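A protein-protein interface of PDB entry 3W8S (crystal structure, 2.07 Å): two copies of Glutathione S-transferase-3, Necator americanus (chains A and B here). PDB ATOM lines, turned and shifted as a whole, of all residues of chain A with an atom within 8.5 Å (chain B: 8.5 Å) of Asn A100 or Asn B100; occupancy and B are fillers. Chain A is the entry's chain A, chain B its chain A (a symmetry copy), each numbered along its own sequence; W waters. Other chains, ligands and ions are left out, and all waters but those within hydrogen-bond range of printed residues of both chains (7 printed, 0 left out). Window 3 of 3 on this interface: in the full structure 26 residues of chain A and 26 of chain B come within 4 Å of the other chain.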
ATOM      1  N   PHE A  65      12.593   9.715  -1.631  1.00  0.00           N
ATOM      2  CA  PHE A  65      12.959  10.094  -0.259  1.00  0.00           C
ATOM      3  C   PHE A  65      12.805   8.975   0.748  1.00  0.00           C
ATOM      4  O   PHE A  65      13.588   8.849   1.707  1.00  0.00           O
ATOM      5  CB  PHE A  65      12.214  11.362   0.215  1.00  0.00           C
ATOM      6  CG  PHE A  65      12.629  12.577  -0.571  1.00  0.00           C
ATOM      7  CD1 PHE A  65      12.106  12.841  -1.840  1.00  0.00           C
ATOM      8  CD2 PHE A  65      13.613  13.412  -0.105  1.00  0.00           C
ATOM      9  CE1 PHE A  65      12.519  13.978  -2.584  1.00  0.00           C
ATOM     10  CE2 PHE A  65      13.986  14.557  -0.808  1.00  0.00           C
ATOM     11  CZ  PHE A  65      13.499  14.816  -2.048  1.00  0.00           C
ATOM     12  N   ASP A  93      11.825  17.438   3.293  1.00  0.00           N
ATOM     13  CA  ASP A  93      10.457  17.739   2.880  1.00  0.00           C
ATOM     14  C   ASP A  93      10.355  19.205   2.378  1.00  0.00           C
ATOM     15  O   ASP A  93       9.643  19.496   1.394  1.00  0.00           O
ATOM     16  CB  ASP A  93       9.473  17.508   4.038  1.00  0.00           C
ATOM     17  CG  ASP A  93       8.976  16.020   4.103  1.00  0.00           C
ATOM     18  OD1 ASP A  93       9.323  15.205   3.193  1.00  0.00           O
ATOM     19  OD2 ASP A  93       8.214  15.694   5.052  1.00  0.00           O
ATOM     20  N   GLN A  94      11.031  20.122   3.047  1.00  0.00           N
ATOM     21  CA  GLN A  94      11.032  21.505   2.517  1.00  0.00           C
ATOM     22  C   GLN A  94      11.677  21.616   1.105  1.00  0.00           C
ATOM     23  O   GLN A  94      11.296  22.451   0.260  1.00  0.00           O
ATOM     24  CB  GLN A  94      11.756  22.466   3.513  1.00  0.00           C
ATOM     25  CG  GLN A  94      11.651  23.990   3.157  1.00  0.00           C
ATOM     26  CD  GLN A  94      10.196  24.502   3.164  1.00  0.00           C
ATOM     27  OE1 GLN A  94       9.287  23.913   3.816  1.00  0.00           O
ATOM     28  NE2 GLN A  94       9.972  25.648   2.504  1.00  0.00           N
ATOM     29  N   TYR A  95      12.764  20.862   0.921  1.00  0.00           N
ATOM     30  CA  TYR A  95      13.471  20.816  -0.341  1.00  0.00           C
ATOM     31  C   TYR A  95      12.498  20.276  -1.438  1.00  0.00           C
ATOM     32  O   TYR A  95      12.430  20.786  -2.544  1.00  0.00           O
ATOM     33  CB  TYR A  95      14.683  19.857  -0.178  1.00  0.00           C
ATOM     34  CG  TYR A  95      15.323  19.517  -1.496  1.00  0.00           C
ATOM     35  CD1 TYR A  95      16.149  20.447  -2.118  1.00  0.00           C
ATOM     36  CD2 TYR A  95      15.076  18.282  -2.156  1.00  0.00           C
ATOM     37  CE1 TYR A  95      16.742  20.193  -3.356  1.00  0.00           C
ATOM     38  CE2 TYR A  95      15.671  18.007  -3.403  1.00  0.00           C
ATOM     39  CZ  TYR A  95      16.521  18.986  -3.967  1.00  0.00           C
ATOM     40  OH  TYR A  95      17.150  18.813  -5.183  1.00  0.00           O
ATOM     41  N   LYS A  96      11.719  19.260  -1.104  1.00  0.00           N
ATOM     42  CA  LYS A  96      10.721  18.762  -2.021  1.00  0.00           C
ATOM     43  C   LYS A  96       9.684  19.864  -2.361  1.00  0.00           C
ATOM     44  O   LYS A  96       9.325  19.989  -3.507  1.00  0.00           O
ATOM     45  CB  LYS A  96      10.050  17.538  -1.414  1.00  0.00           C
ATOM     46  CG  LYS A  96       8.789  17.047  -2.129  1.00  0.00           C
ATOM     47  CD  LYS A  96       8.326  15.700  -1.457  1.00  0.00           C
ATOM     48  CE  LYS A  96       9.055  14.506  -2.075  1.00  0.00           C
ATOM     49  NZ  LYS A  96       8.664  13.154  -1.609  1.00  0.00           N
ATOM     50  N   ASP A  97       9.219  20.652  -1.375  1.00  0.00           N
ATOM     51  CA  ASP A  97       8.363  21.787  -1.674  1.00  0.00           C
ATOM     52  C   ASP A  97       9.055  22.781  -2.625  1.00  0.00           C
ATOM     53  O   ASP A  97       8.417  23.332  -3.486  1.00  0.00           O
ATOM     54  CB  ASP A  97       7.889  22.553  -0.403  1.00  0.00           C
ATOM     55  CG  ASP A  97       6.907  21.749   0.456  1.00  0.00           C
ATOM     56  OD1 ASP A  97       6.316  20.729  -0.013  1.00  0.00           O
ATOM     57  OD2 ASP A  97       6.687  22.177   1.628  1.00  0.00           O
ATOM     58  N   PHE A  98      10.337  23.051  -2.412  1.00  0.00           N
ATOM     59  CA  PHE A  98      11.074  24.054  -3.206  1.00  0.00           C
ATOM     60  C   PHE A  98      11.100  23.472  -4.664  1.00  0.00           C
ATOM     61  O   PHE A  98      10.835  24.199  -5.623  1.00  0.00           O
ATOM     62  CB  PHE A  98      12.458  24.163  -2.599  1.00  0.00           C
ATOM     63  CG  PHE A  98      13.486  24.699  -3.526  1.00  0.00           C
ATOM     64  CD1 PHE A  98      13.365  26.032  -4.044  1.00  0.00           C
ATOM     65  CD2 PHE A  98      14.599  23.917  -3.896  1.00  0.00           C
ATOM     66  CE1 PHE A  98      14.331  26.542  -4.908  1.00  0.00           C
ATOM     67  CE2 PHE A  98      15.614  24.454  -4.787  1.00  0.00           C
ATOM     68  CZ  PHE A  98      15.451  25.766  -5.297  1.00  0.00           C
ATOM     69  N   ILE A  99      11.435  22.180  -4.804  1.00  0.00           N
ATOM     70  CA  ILE A  99      11.463  21.522  -6.136  1.00  0.00           C
ATOM     71  C   ILE A  99      10.107  21.616  -6.842  1.00  0.00           C
ATOM     72  O   ILE A  99      10.047  21.972  -8.043  1.00  0.00           O
ATOM     73  CB  ILE A  99      11.984  20.042  -6.068  1.00  0.00           C
ATOM     74  CG1 ILE A  99      13.451  20.069  -5.575  1.00  0.00           C
ATOM     75  CG2 ILE A  99      11.865  19.360  -7.458  1.00  0.00           C
ATOM     76  CD1 ILE A  99      14.341  20.875  -6.503  1.00  0.00           C
ATOM     77  N   ASN A 100       9.025  21.342  -6.109  1.00  0.00           N
ATOM     78  CA  ASN A 100       7.679  21.497  -6.655  1.00  0.00           C
ATOM     79  C   ASN A 100       7.406  22.967  -7.059  1.00  0.00           C
ATOM     80  O   ASN A 100       6.771  23.209  -8.058  1.00  0.00           O
ATOM     81  CB  ASN A 100       6.596  20.911  -5.683  1.00  0.00           C
ATOM     82  CG  ASN A 100       6.626  19.341  -5.637  1.00  0.00           C
ATOM     83  OD1 ASN A 100       6.944  18.691  -6.634  1.00  0.00           O
ATOM     84  ND2 ASN A 100       6.298  18.740  -4.479  1.00  0.00           N
ATOM     85  N   GLU A 101       7.930  23.934  -6.312  1.00  0.00           N
ATOM     86  CA  GLU A 101       7.642  25.304  -6.593  1.00  0.00           C
ATOM     87  C   GLU A 101       8.355  25.754  -7.927  1.00  0.00           C
ATOM     88  O   GLU A 101       7.801  26.537  -8.686  1.00  0.00           O
ATOM     89  CB  GLU A 101       8.072  26.193  -5.424  1.00  0.00           C
ATOM     90  CG  GLU A 101       7.808  27.652  -5.656  1.00  0.00           C
ATOM     91  CD  GLU A 101       8.321  28.547  -4.505  1.00  0.00           C
ATOM     92  OE1 GLU A 101       8.884  28.029  -3.518  1.00  0.00           O
ATOM     93  OE2 GLU A 101       8.184  29.766  -4.590  1.00  0.00           O
ATOM     94  N   ILE A 102       9.538  25.253  -8.193  1.00  0.00           N
ATOM     95  CA  ILE A 102      10.243  25.652  -9.394  1.00  0.00           C
ATOM     96  C   ILE A 102       9.960  24.755 -10.613  1.00  0.00           C
ATOM     97  O   ILE A 102      10.636  24.849 -11.627  1.00  0.00           O
ATOM     98  CB  ILE A 102      11.723  25.766  -9.128  1.00  0.00           C
ATOM     99  CG1 ILE A 102      12.296  24.370  -8.790  1.00  0.00           C
ATOM    100  CG2 ILE A 102      11.946  26.743  -7.950  1.00  0.00           C
ATOM    101  CD1 ILE A 102      13.819  24.350  -8.757  1.00  0.00           C
ATOM    102  N   ARG A 103       8.978  23.879 -10.496  1.00  0.00           N
ATOM    103  CA  ARG A 103       8.550  23.024 -11.599  1.00  0.00           C
ATOM    104  C   ARG A 103       8.449  23.758 -12.952  1.00  0.00           C
ATOM    105  O   ARG A 103       9.013  23.265 -13.916  1.00  0.00           O
ATOM    106  CB  ARG A 103       7.176  22.411 -11.297  1.00  0.00           C
ATOM    107  CG  ARG A 103       6.788  21.363 -12.327  1.00  0.00           C
ATOM    108  CD  ARG A 103       5.507  20.637 -11.955  1.00  0.00           C
ATOM    109  NE  ARG A 103       5.365  19.472 -12.823  1.00  0.00           N
ATOM    110  CZ  ARG A 103       4.664  19.466 -13.954  1.00  0.00           C
ATOM    111  NH1 ARG A 103       4.031  20.566 -14.352  1.00  0.00           N
ATOM    112  NH2 ARG A 103       4.595  18.364 -14.681  1.00  0.00           N
ATOM    113  N   PRO A 104       7.734  24.912 -13.025  1.00  0.00           N
ATOM    114  CA  PRO A 104       7.571  25.623 -14.293  1.00  0.00           C
ATOM    115  C   PRO A 104       8.937  25.968 -14.912  1.00  0.00           C
ATOM    116  O   PRO A 104       9.101  25.868 -16.144  1.00  0.00           O
ATOM    117  CB  PRO A 104       6.866  26.939 -13.884  1.00  0.00           C
ATOM    118  CG  PRO A 104       6.107  26.584 -12.662  1.00  0.00           C
ATOM    119  CD  PRO A 104       7.063  25.655 -11.925  1.00  0.00           C
ATOM    120  N   PHE A 105       9.905  26.341 -14.071  1.00  0.00           N
ATOM    121  CA  PHE A 105      11.257  26.610 -14.525  1.00  0.00           C
ATOM    122  C   PHE A 105      11.896  25.328 -14.967  1.00  0.00           C
ATOM    123  O   PHE A 105      12.539  25.268 -16.062  1.00  0.00           O
ATOM    124  CB  PHE A 105      12.111  27.300 -13.432  1.00  0.00           C
ATOM    125  CG  PHE A 105      13.596  27.299 -13.688  1.00  0.00           C
ATOM    126  CD1 PHE A 105      14.186  28.239 -14.569  1.00  0.00           C
ATOM    127  CD2 PHE A 105      14.396  26.473 -13.004  1.00  0.00           C
ATOM    128  CE1 PHE A 105      15.544  28.272 -14.785  1.00  0.00           C
ATOM    129  CE2 PHE A 105      15.778  26.479 -13.194  1.00  0.00           C
ATOM    130  CZ  PHE A 105      16.370  27.380 -14.095  1.00  0.00           C
ATOM    131  N   LEU A 106      11.770  24.295 -14.140  1.00  0.00           N
ATOM    132  CA  LEU A 106      12.513  23.063 -14.500  1.00  0.00           C
ATOM    133  C   LEU A 106      11.983  22.388 -15.809  1.00  0.00           C
ATOM    134  O   LEU A 106      12.737  21.811 -16.555  1.00  0.00           O
ATOM    135  CB  LEU A 106      12.537  22.083 -13.325  1.00  0.00           C
ATOM    136  CG  LEU A 106      13.349  22.434 -12.083  1.00  0.00           C
ATOM    137  CD1 LEU A 106      12.950  21.487 -10.961  1.00  0.00           C
ATOM    138  CD2 LEU A 106      14.831  22.315 -12.330  1.00  0.00           C
ATOM    139  N   VAL A 124      10.686  32.778 -11.184  1.00  0.00           N
ATOM    140  CA  VAL A 124      10.284  31.556 -10.471  1.00  0.00           C
ATOM    141  C   VAL A 124      11.508  30.969  -9.722  1.00  0.00           C
ATOM    142  O   VAL A 124      11.469  30.790  -8.501  1.00  0.00           O
ATOM    143  CB  VAL A 124       9.654  30.482 -11.401  1.00  0.00           C
ATOM    144  CG1 VAL A 124       9.363  29.175 -10.624  1.00  0.00           C
ATOM    145  CG2 VAL A 124       8.325  31.007 -11.986  1.00  0.00           C
ATOM    146  N   ALA A 128      12.252  31.586  -5.610  1.00  0.00           N
ATOM    147  CA  ALA A 128      12.058  30.369  -4.802  1.00  0.00           C
ATOM    148  C   ALA A 128      13.335  30.008  -4.053  1.00  0.00           C
ATOM    149  O   ALA A 128      13.206  29.663  -2.892  1.00  0.00           O
ATOM    150  CB  ALA A 128      11.612  29.176  -5.677  1.00  0.00           C
ATOM    151  N   PHE B  65       4.677  15.642   7.352  1.00  0.00           N
ATOM    152  CA  PHE B  65       5.070  14.227   7.333  1.00  0.00           C
ATOM    153  C   PHE B  65       6.273  13.912   8.196  1.00  0.00           C
ATOM    154  O   PHE B  65       6.371  12.833   8.809  1.00  0.00           O
ATOM    155  CB  PHE B  65       5.275  13.696   5.896  1.00  0.00           C
ATOM    156  CG  PHE B  65       3.985  13.677   5.121  1.00  0.00           C
ATOM    157  CD1 PHE B  65       3.466  14.836   4.535  1.00  0.00           C
ATOM    158  CD2 PHE B  65       3.223  12.538   5.053  1.00  0.00           C
ATOM    159  CE1 PHE B  65       2.238  14.815   3.824  1.00  0.00           C
ATOM    160  CE2 PHE B  65       2.042  12.499   4.313  1.00  0.00           C
ATOM    161  CZ  PHE B  65       1.519  13.620   3.754  1.00  0.00           C
ATOM    162  N   ASP B  93       4.604   9.069   0.928  1.00  0.00           N
ATOM    163  CA  ASP B  93       5.140   9.905  -0.143  1.00  0.00           C
ATOM    164  C   ASP B  93       4.249   9.796  -1.410  1.00  0.00           C
ATOM    165  O   ASP B  93       4.014  10.800  -2.115  1.00  0.00           O
ATOM    166  CB  ASP B  93       6.585   9.505  -0.477  1.00  0.00           C
ATOM    167  CG  ASP B  93       7.629  10.246   0.432  1.00  0.00           C
ATOM    168  OD1 ASP B  93       7.229  11.134   1.247  1.00  0.00           O
ATOM    169  OD2 ASP B  93       8.846   9.950   0.295  1.00  0.00           O
ATOM    170  N   GLN B  94       3.777   8.600  -1.716  1.00  0.00           N
ATOM    171  CA  GLN B  94       2.839   8.498  -2.857  1.00  0.00           C
ATOM    172  C   GLN B  94       1.524   9.303  -2.639  1.00  0.00           C
ATOM    173  O   GLN B  94       0.904   9.837  -3.580  1.00  0.00           O
ATOM    174  CB  GLN B  94       2.507   7.001  -3.153  1.00  0.00           C
ATOM    175  CG  GLN B  94       1.679   6.753  -4.462  1.00  0.00           C
ATOM    176  CD  GLN B  94       2.425   7.209  -5.732  1.00  0.00           C
ATOM    177  OE1 GLN B  94       3.684   7.320  -5.760  1.00  0.00           O
ATOM    178  NE2 GLN B  94       1.667   7.405  -6.823  1.00  0.00           N
ATOM    179  N   TYR B  95       1.028   9.248  -1.400  1.00  0.00           N
ATOM    180  CA  TYR B  95      -0.168   9.963  -1.011  1.00  0.00           C
ATOM    181  C   TYR B  95       0.080  11.494  -1.205  1.00  0.00           C
ATOM    182  O   TYR B  95      -0.757  12.221  -1.714  1.00  0.00           O
ATOM    183  CB  TYR B  95      -0.449   9.650   0.485  1.00  0.00           C
ATOM    184  CG  TYR B  95      -1.501  10.554   1.069  1.00  0.00           C
ATOM    185  CD1 TYR B  95      -2.841  10.326   0.774  1.00  0.00           C
ATOM    186  CD2 TYR B  95      -1.166  11.669   1.885  1.00  0.00           C
ATOM    187  CE1 TYR B  95      -3.853  11.152   1.265  1.00  0.00           C
ATOM    188  CE2 TYR B  95      -2.176  12.510   2.393  1.00  0.00           C
ATOM    189  CZ  TYR B  95      -3.520  12.206   2.076  1.00  0.00           C
ATOM    190  OH  TYR B  95      -4.580  12.968   2.524  1.00  0.00           O
ATOM    191  N   LYS B  96       1.258  11.965  -0.829  1.00  0.00           N
ATOM    192  CA  LYS B  96       1.610  13.345  -1.063  1.00  0.00           C
ATOM    193  C   LYS B  96       1.606  13.667  -2.581  1.00  0.00           C
ATOM    194  O   LYS B  96       1.114  14.705  -2.952  1.00  0.00           O
ATOM    195  CB  LYS B  96       2.971  13.627  -0.442  1.00  0.00           C
ATOM    196  CG  LYS B  96       3.615  14.961  -0.826  1.00  0.00           C
ATOM    197  CD  LYS B  96       4.930  15.143   0.021  1.00  0.00           C
ATOM    198  CE  LYS B  96       4.618  15.769   1.382  1.00  0.00           C
ATOM    199  NZ  LYS B  96       5.765  16.086   2.265  1.00  0.00           N
ATOM    200  N   ASP B  97       2.142  12.781  -3.439  1.00  0.00           N
ATOM    201  CA  ASP B  97       2.026  12.976  -4.874  1.00  0.00           C
ATOM    202  C   ASP B  97       0.552  13.049  -5.317  1.00  0.00           C
ATOM    203  O   ASP B  97       0.223  13.821  -6.181  1.00  0.00           O
ATOM    204  CB  ASP B  97       2.746  11.873  -5.706  1.00  0.00           C
ATOM    205  CG  ASP B  97       4.273  11.932  -5.593  1.00  0.00           C
ATOM    206  OD1 ASP B  97       4.854  12.966  -5.143  1.00  0.00           O
ATOM    207  OD2 ASP B  97       4.919  10.923  -6.007  1.00  0.00           O
ATOM    208  N   PHE B  98      -0.302  12.195  -4.767  1.00  0.00           N
ATOM    209  CA  PHE B  98      -1.717  12.118  -5.181  1.00  0.00           C
ATOM    210  C   PHE B  98      -2.330  13.504  -4.773  1.00  0.00           C
ATOM    211  O   PHE B  98      -3.048  14.119  -5.564  1.00  0.00           O
ATOM    212  CB  PHE B  98      -2.334  10.962  -4.422  1.00  0.00           C
ATOM    213  CG  PHE B  98      -3.811  11.039  -4.295  1.00  0.00           C
ATOM    214  CD1 PHE B  98      -4.638  11.002  -5.468  1.00  0.00           C
ATOM    215  CD2 PHE B  98      -4.420  11.133  -3.028  1.00  0.00           C
ATOM    216  CE1 PHE B  98      -6.025  11.067  -5.354  1.00  0.00           C
ATOM    217  CE2 PHE B  98      -5.868  11.187  -2.908  1.00  0.00           C
ATOM    218  CZ  PHE B  98      -6.653  11.170  -4.087  1.00  0.00           C
ATOM    219  N   ILE B  99      -2.053  13.959  -3.541  1.00  0.00           N
ATOM    220  CA  ILE B  99      -2.561  15.271  -3.062  1.00  0.00           C
ATOM    221  C   ILE B  99      -2.112  16.418  -3.974  1.00  0.00           C
ATOM    222  O   ILE B  99      -2.941  17.276  -4.358  1.00  0.00           O
ATOM    223  CB  ILE B  99      -2.199  15.547  -1.559  1.00  0.00           C
ATOM    224  CG1 ILE B  99      -2.904  14.476  -0.690  1.00  0.00           C
ATOM    225  CG2 ILE B  99      -2.632  16.981  -1.151  1.00  0.00           C
ATOM    226  CD1 ILE B  99      -4.410  14.514  -0.863  1.00  0.00           C
ATOM    227  N   ASN B 100      -0.831  16.421  -4.354  1.00  0.00           N
ATOM    228  CA  ASN B 100      -0.323  17.410  -5.300  1.00  0.00           C
ATOM    229  C   ASN B 100      -1.043  17.296  -6.667  1.00  0.00           C
ATOM    230  O   ASN B 100      -1.317  18.297  -7.288  1.00  0.00           O
ATOM    231  CB  ASN B 100       1.240  17.340  -5.417  1.00  0.00           C
ATOM    232  CG  ASN B 100       1.957  17.890  -4.131  1.00  0.00           C
ATOM    233  OD1 ASN B 100       1.450  18.798  -3.471  1.00  0.00           O
ATOM    234  ND2 ASN B 100       3.131  17.334  -3.781  1.00  0.00           N
ATOM    235  N   GLU B 101      -1.390  16.089  -7.099  1.00  0.00           N
ATOM    236  CA  GLU B 101      -1.983  15.921  -8.387  1.00  0.00           C
ATOM    237  C   GLU B 101      -3.449  16.502  -8.398  1.00  0.00           C
ATOM    238  O   GLU B 101      -3.880  17.065  -9.395  1.00  0.00           O
ATOM    239  CB  GLU B 101      -1.982  14.446  -8.790  1.00  0.00           C
ATOM    240  CG  GLU B 101      -2.602  14.194 -10.133  1.00  0.00           C
ATOM    241  CD  GLU B 101      -2.671  12.692 -10.493  1.00  0.00           C
ATOM    242  OE1 GLU B 101      -2.232  11.840  -9.693  1.00  0.00           O
ATOM    243  OE2 GLU B 101      -3.181  12.357 -11.560  1.00  0.00           O
ATOM    244  N   ILE B 102      -4.172  16.373  -7.311  1.00  0.00           N
ATOM    245  CA  ILE B 102      -5.532  16.870  -7.278  1.00  0.00           C
ATOM    246  C   ILE B 102      -5.656  18.324  -6.785  1.00  0.00           C
ATOM    247  O   ILE B 102      -6.749  18.800  -6.514  1.00  0.00           O
ATOM    248  CB  ILE B 102      -6.417  15.943  -6.483  1.00  0.00           C
ATOM    249  CG1 ILE B 102      -5.971  15.946  -5.003  1.00  0.00           C
ATOM    250  CG2 ILE B 102      -6.313  14.520  -7.079  1.00  0.00           C
ATOM    251  CD1 ILE B 102      -6.961  15.238  -4.087  1.00  0.00           C
ATOM    252  N   ARG B 103      -4.533  19.008  -6.652  1.00  0.00           N
ATOM    253  CA  ARG B 103      -4.511  20.417  -6.272  1.00  0.00           C
ATOM    254  C   ARG B 103      -5.574  21.273  -6.992  1.00  0.00           C
ATOM    255  O   ARG B 103      -6.297  21.983  -6.312  1.00  0.00           O
ATOM    256  CB  ARG B 103      -3.136  21.029  -6.572  1.00  0.00           C
ATOM    257  CG  ARG B 103      -3.011  22.435  -6.010  1.00  0.00           C
ATOM    258  CD  ARG B 103      -1.606  22.992  -6.161  1.00  0.00           C
ATOM    259  NE  ARG B 103      -1.496  24.201  -5.350  1.00  0.00           N
ATOM    260  CZ  ARG B 103      -1.691  25.432  -5.817  1.00  0.00           C
ATOM    261  NH1 ARG B 103      -1.999  25.618  -7.097  1.00  0.00           N
ATOM    262  NH2 ARG B 103      -1.575  26.470  -5.006  1.00  0.00           N
ATOM    263  N   PRO B 104      -5.659  21.213  -8.348  1.00  0.00           N
ATOM    264  CA  PRO B 104      -6.620  22.037  -9.083  1.00  0.00           C
ATOM    265  C   PRO B 104      -8.055  21.787  -8.587  1.00  0.00           C
ATOM    266  O   PRO B 104      -8.845  22.744  -8.473  1.00  0.00           O
ATOM    267  CB  PRO B 104      -6.502  21.523 -10.538  1.00  0.00           C
ATOM    268  CG  PRO B 104      -5.112  21.018 -10.636  1.00  0.00           C
ATOM    269  CD  PRO B 104      -4.898  20.347  -9.286  1.00  0.00           C
ATOM    270  N   PHE B 105      -8.375  20.529  -8.273  1.00  0.00           N
ATOM    271  CA  PHE B 105      -9.669  20.182  -7.716  1.00  0.00           C
ATOM    272  C   PHE B 105      -9.778  20.739  -6.329  1.00  0.00           C
ATOM    273  O   PHE B 105     -10.827  21.353  -5.957  1.00  0.00           O
ATOM    274  CB  PHE B 105      -9.908  18.651  -7.712  1.00  0.00           C
ATOM    275  CG  PHE B 105     -11.053  18.186  -6.849  1.00  0.00           C
ATOM    276  CD1 PHE B 105     -12.392  18.270  -7.304  1.00  0.00           C
ATOM    277  CD2 PHE B 105     -10.811  17.589  -5.676  1.00  0.00           C
ATOM    278  CE1 PHE B 105     -13.443  17.817  -6.541  1.00  0.00           C
ATOM    279  CE2 PHE B 105     -11.851  17.116  -4.876  1.00  0.00           C
ATOM    280  CZ  PHE B 105     -13.186  17.230  -5.300  1.00  0.00           C
ATOM    281  N   LEU B 106      -8.739  20.524  -5.528  1.00  0.00           N
ATOM    282  CA  LEU B 106      -8.892  20.949  -4.116  1.00  0.00           C
ATOM    283  C   LEU B 106      -9.004  22.501  -3.952  1.00  0.00           C
ATOM    284  O   LEU B 106      -9.687  22.983  -3.080  1.00  0.00           O
ATOM    285  CB  LEU B 106      -7.772  20.365  -3.252  1.00  0.00           C
ATOM    286  CG  LEU B 106      -7.742  18.864  -2.992  1.00  0.00           C
ATOM    287  CD1 LEU B 106      -6.386  18.502  -2.405  1.00  0.00           C
ATOM    288  CD2 LEU B 106      -8.826  18.438  -2.033  1.00  0.00           C
ATOM    289  N   VAL B 124     -10.105  15.389 -12.852  1.00  0.00           N
ATOM    290  CA  VAL B 124      -8.863  15.463 -12.068  1.00  0.00           C
ATOM    291  C   VAL B 124      -8.976  14.531 -10.834  1.00  0.00           C
ATOM    292  O   VAL B 124      -8.149  13.633 -10.651  1.00  0.00           O
ATOM    293  CB  VAL B 124      -8.504  16.908 -11.621  1.00  0.00           C
ATOM    294  CG1 VAL B 124      -7.261  16.913 -10.700  1.00  0.00           C
ATOM    295  CG2 VAL B 124      -8.197  17.779 -12.858  1.00  0.00           C
ATOM    296  N   ALA B 128      -7.327  10.645 -10.682  1.00  0.00           N
ATOM    297  CA  ALA B 128      -6.171  10.546  -9.773  1.00  0.00           C
ATOM    298  C   ALA B 128      -6.421   9.503  -8.691  1.00  0.00           C
ATOM    299  O   ALA B 128      -5.494   8.758  -8.429  1.00  0.00           O
ATOM    300  CB  ALA B 128      -5.849  11.909  -9.120  1.00  0.00           C
HETATM  301  O   HOH W   1       5.976  16.869   5.072  1.00  0.00           O
HETATM  302  O   HOH W   2       6.247  12.587  -2.692  1.00  0.00           O
HETATM  303  O   HOH W   3       4.555  15.807  -5.031  1.00  0.00           O
HETATM  304  O   HOH W   4       5.298  19.688  -2.473  1.00  0.00           O
HETATM  305  O   HOH W   5       9.824  10.497  -1.970  1.00  0.00           O
HETATM  306  O   HOH W   6       7.806  13.812   1.382  1.00  0.00           O
HETATM  307  O   HOH W   7       7.000  18.269   1.241  1.00  0.00           O
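Of the 17 printed residues of chain A, 4 touch a printed residue of chain B. Printed residues of chain A that touch a printed residue of chain B: Phe A65, Asp A93, Lys A96 and Asn A100. Hydrophobic or aromatic side chains of chain A that line the printed part of chain B: Phe A65. Hydrophobic or aromatic side chains of chain B within 4 Å of the printed part of chain A: Phe B65.
The side-chain carboxylate of Asp A93 is in salt-bridge range of the side-chain amino group of Lys B96. The side-chain carboxylate of Asp B93 is in salt-bridge range of the side-chain amino group of Lys A96 (3.7 Å).
Phe A65 touches Asp B93, and with the chains exchanged Asp A93 touches Phe B65. Asp A93 touches Lys B96, and with the chains exchanged Lys A96 touches Asp B93. Lys A96 touches its own counterpart, Lys B96. Asn B100 touches its own counterpart, Asn A100. Positions printed for both chains: 65, 93, 94, 95, 96, 97, 98, 99, 100, 101, 102, 103, 104, 105, 106, 124 and 128. Of the 6 pairs that touch across the chains among the printed residues, 6 have their exchanged pair printed and touching as well.
Water W4 lies within hydrogen-bond range of the side-chain amide nitrogen of Asn A100, the side-chain carboxylate of Asp A97 and the side-chain amide nitrogen of Asn B100. Water W3 lies within hydrogen-bond range of the side-chain amide nitrogen (ND2) of Asn B100, the side-chain carboxylate (OD1) of Asp B97 and the side-chain amide nitrogen (ND2) of Asn A100. Water W5 lies within hydrogen-bond range of OD2 of Asp B93 (2.5 Å), N of Phe A65 (2.9 Å) and NZ of Lys A96 (2.9 Å). Water W1 lies within hydrogen-bond range of the side-chain carboxylate of Asp A93 (2.5 Å), the backbone NH of Phe B65 (2.9 Å) and the side-chain amino group of Lys B96 (2.9 Å). Water W7 lies within hydrogen-bond range of NZ of Lys B96 (2.7 Å), OD1 of Asp A97 (2.8 Å) and O of Asp A93 (2.9 Å). Water W6 lies within hydrogen-bond range of the side-chain carboxylate of Asp A93 (2.7 Å), the side-chain carboxylate of Asp B93 (2.7 Å), the side-chain amino group of Lys A96 (3.2 Å) and the side-chain amino group of Lys B96 (3.2 Å).
The backbone carbonyl oxygen (O) of Lys A96 is in hydrogen-bond range of the side-chain amide nitrogen (ND2) of Asn A100, 3.4 Å away. The backbone carbonyl oxygen (O) of Lys B96 sits at hydrogen-bond distance from the side-chain amide nitrogen (ND2) of Asn B100 (3.4 Å).
Printed residues of chain A within 4 Å of Asp B93: Phe A65 and Lys A96. Printed residues of chain B within 4 Å of Lys A96: Asp B93 and Lys B96. Arg B103 touches none of the printed residues of chain A. The nearest printed residue of chain B that does not touch Asn A100 is Lys B96 (5.9 Å). The nearest printed residue of chain A that does not touch Asn B100 is Lys A96 (5.9 Å). The nearest printed residue of chain B that does not touch Lys A96 is Asp B97 (5.2 Å).
Asp B93 touches Phe A65 (OD2 to CB, 3.7 Å). Asp A93 touches Phe B65. Lys A96 touches Lys B96 (CD to CD, 3.7 Å). Asn A100 touches Asn B100 (ND2 to ND2, 3.5 Å).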
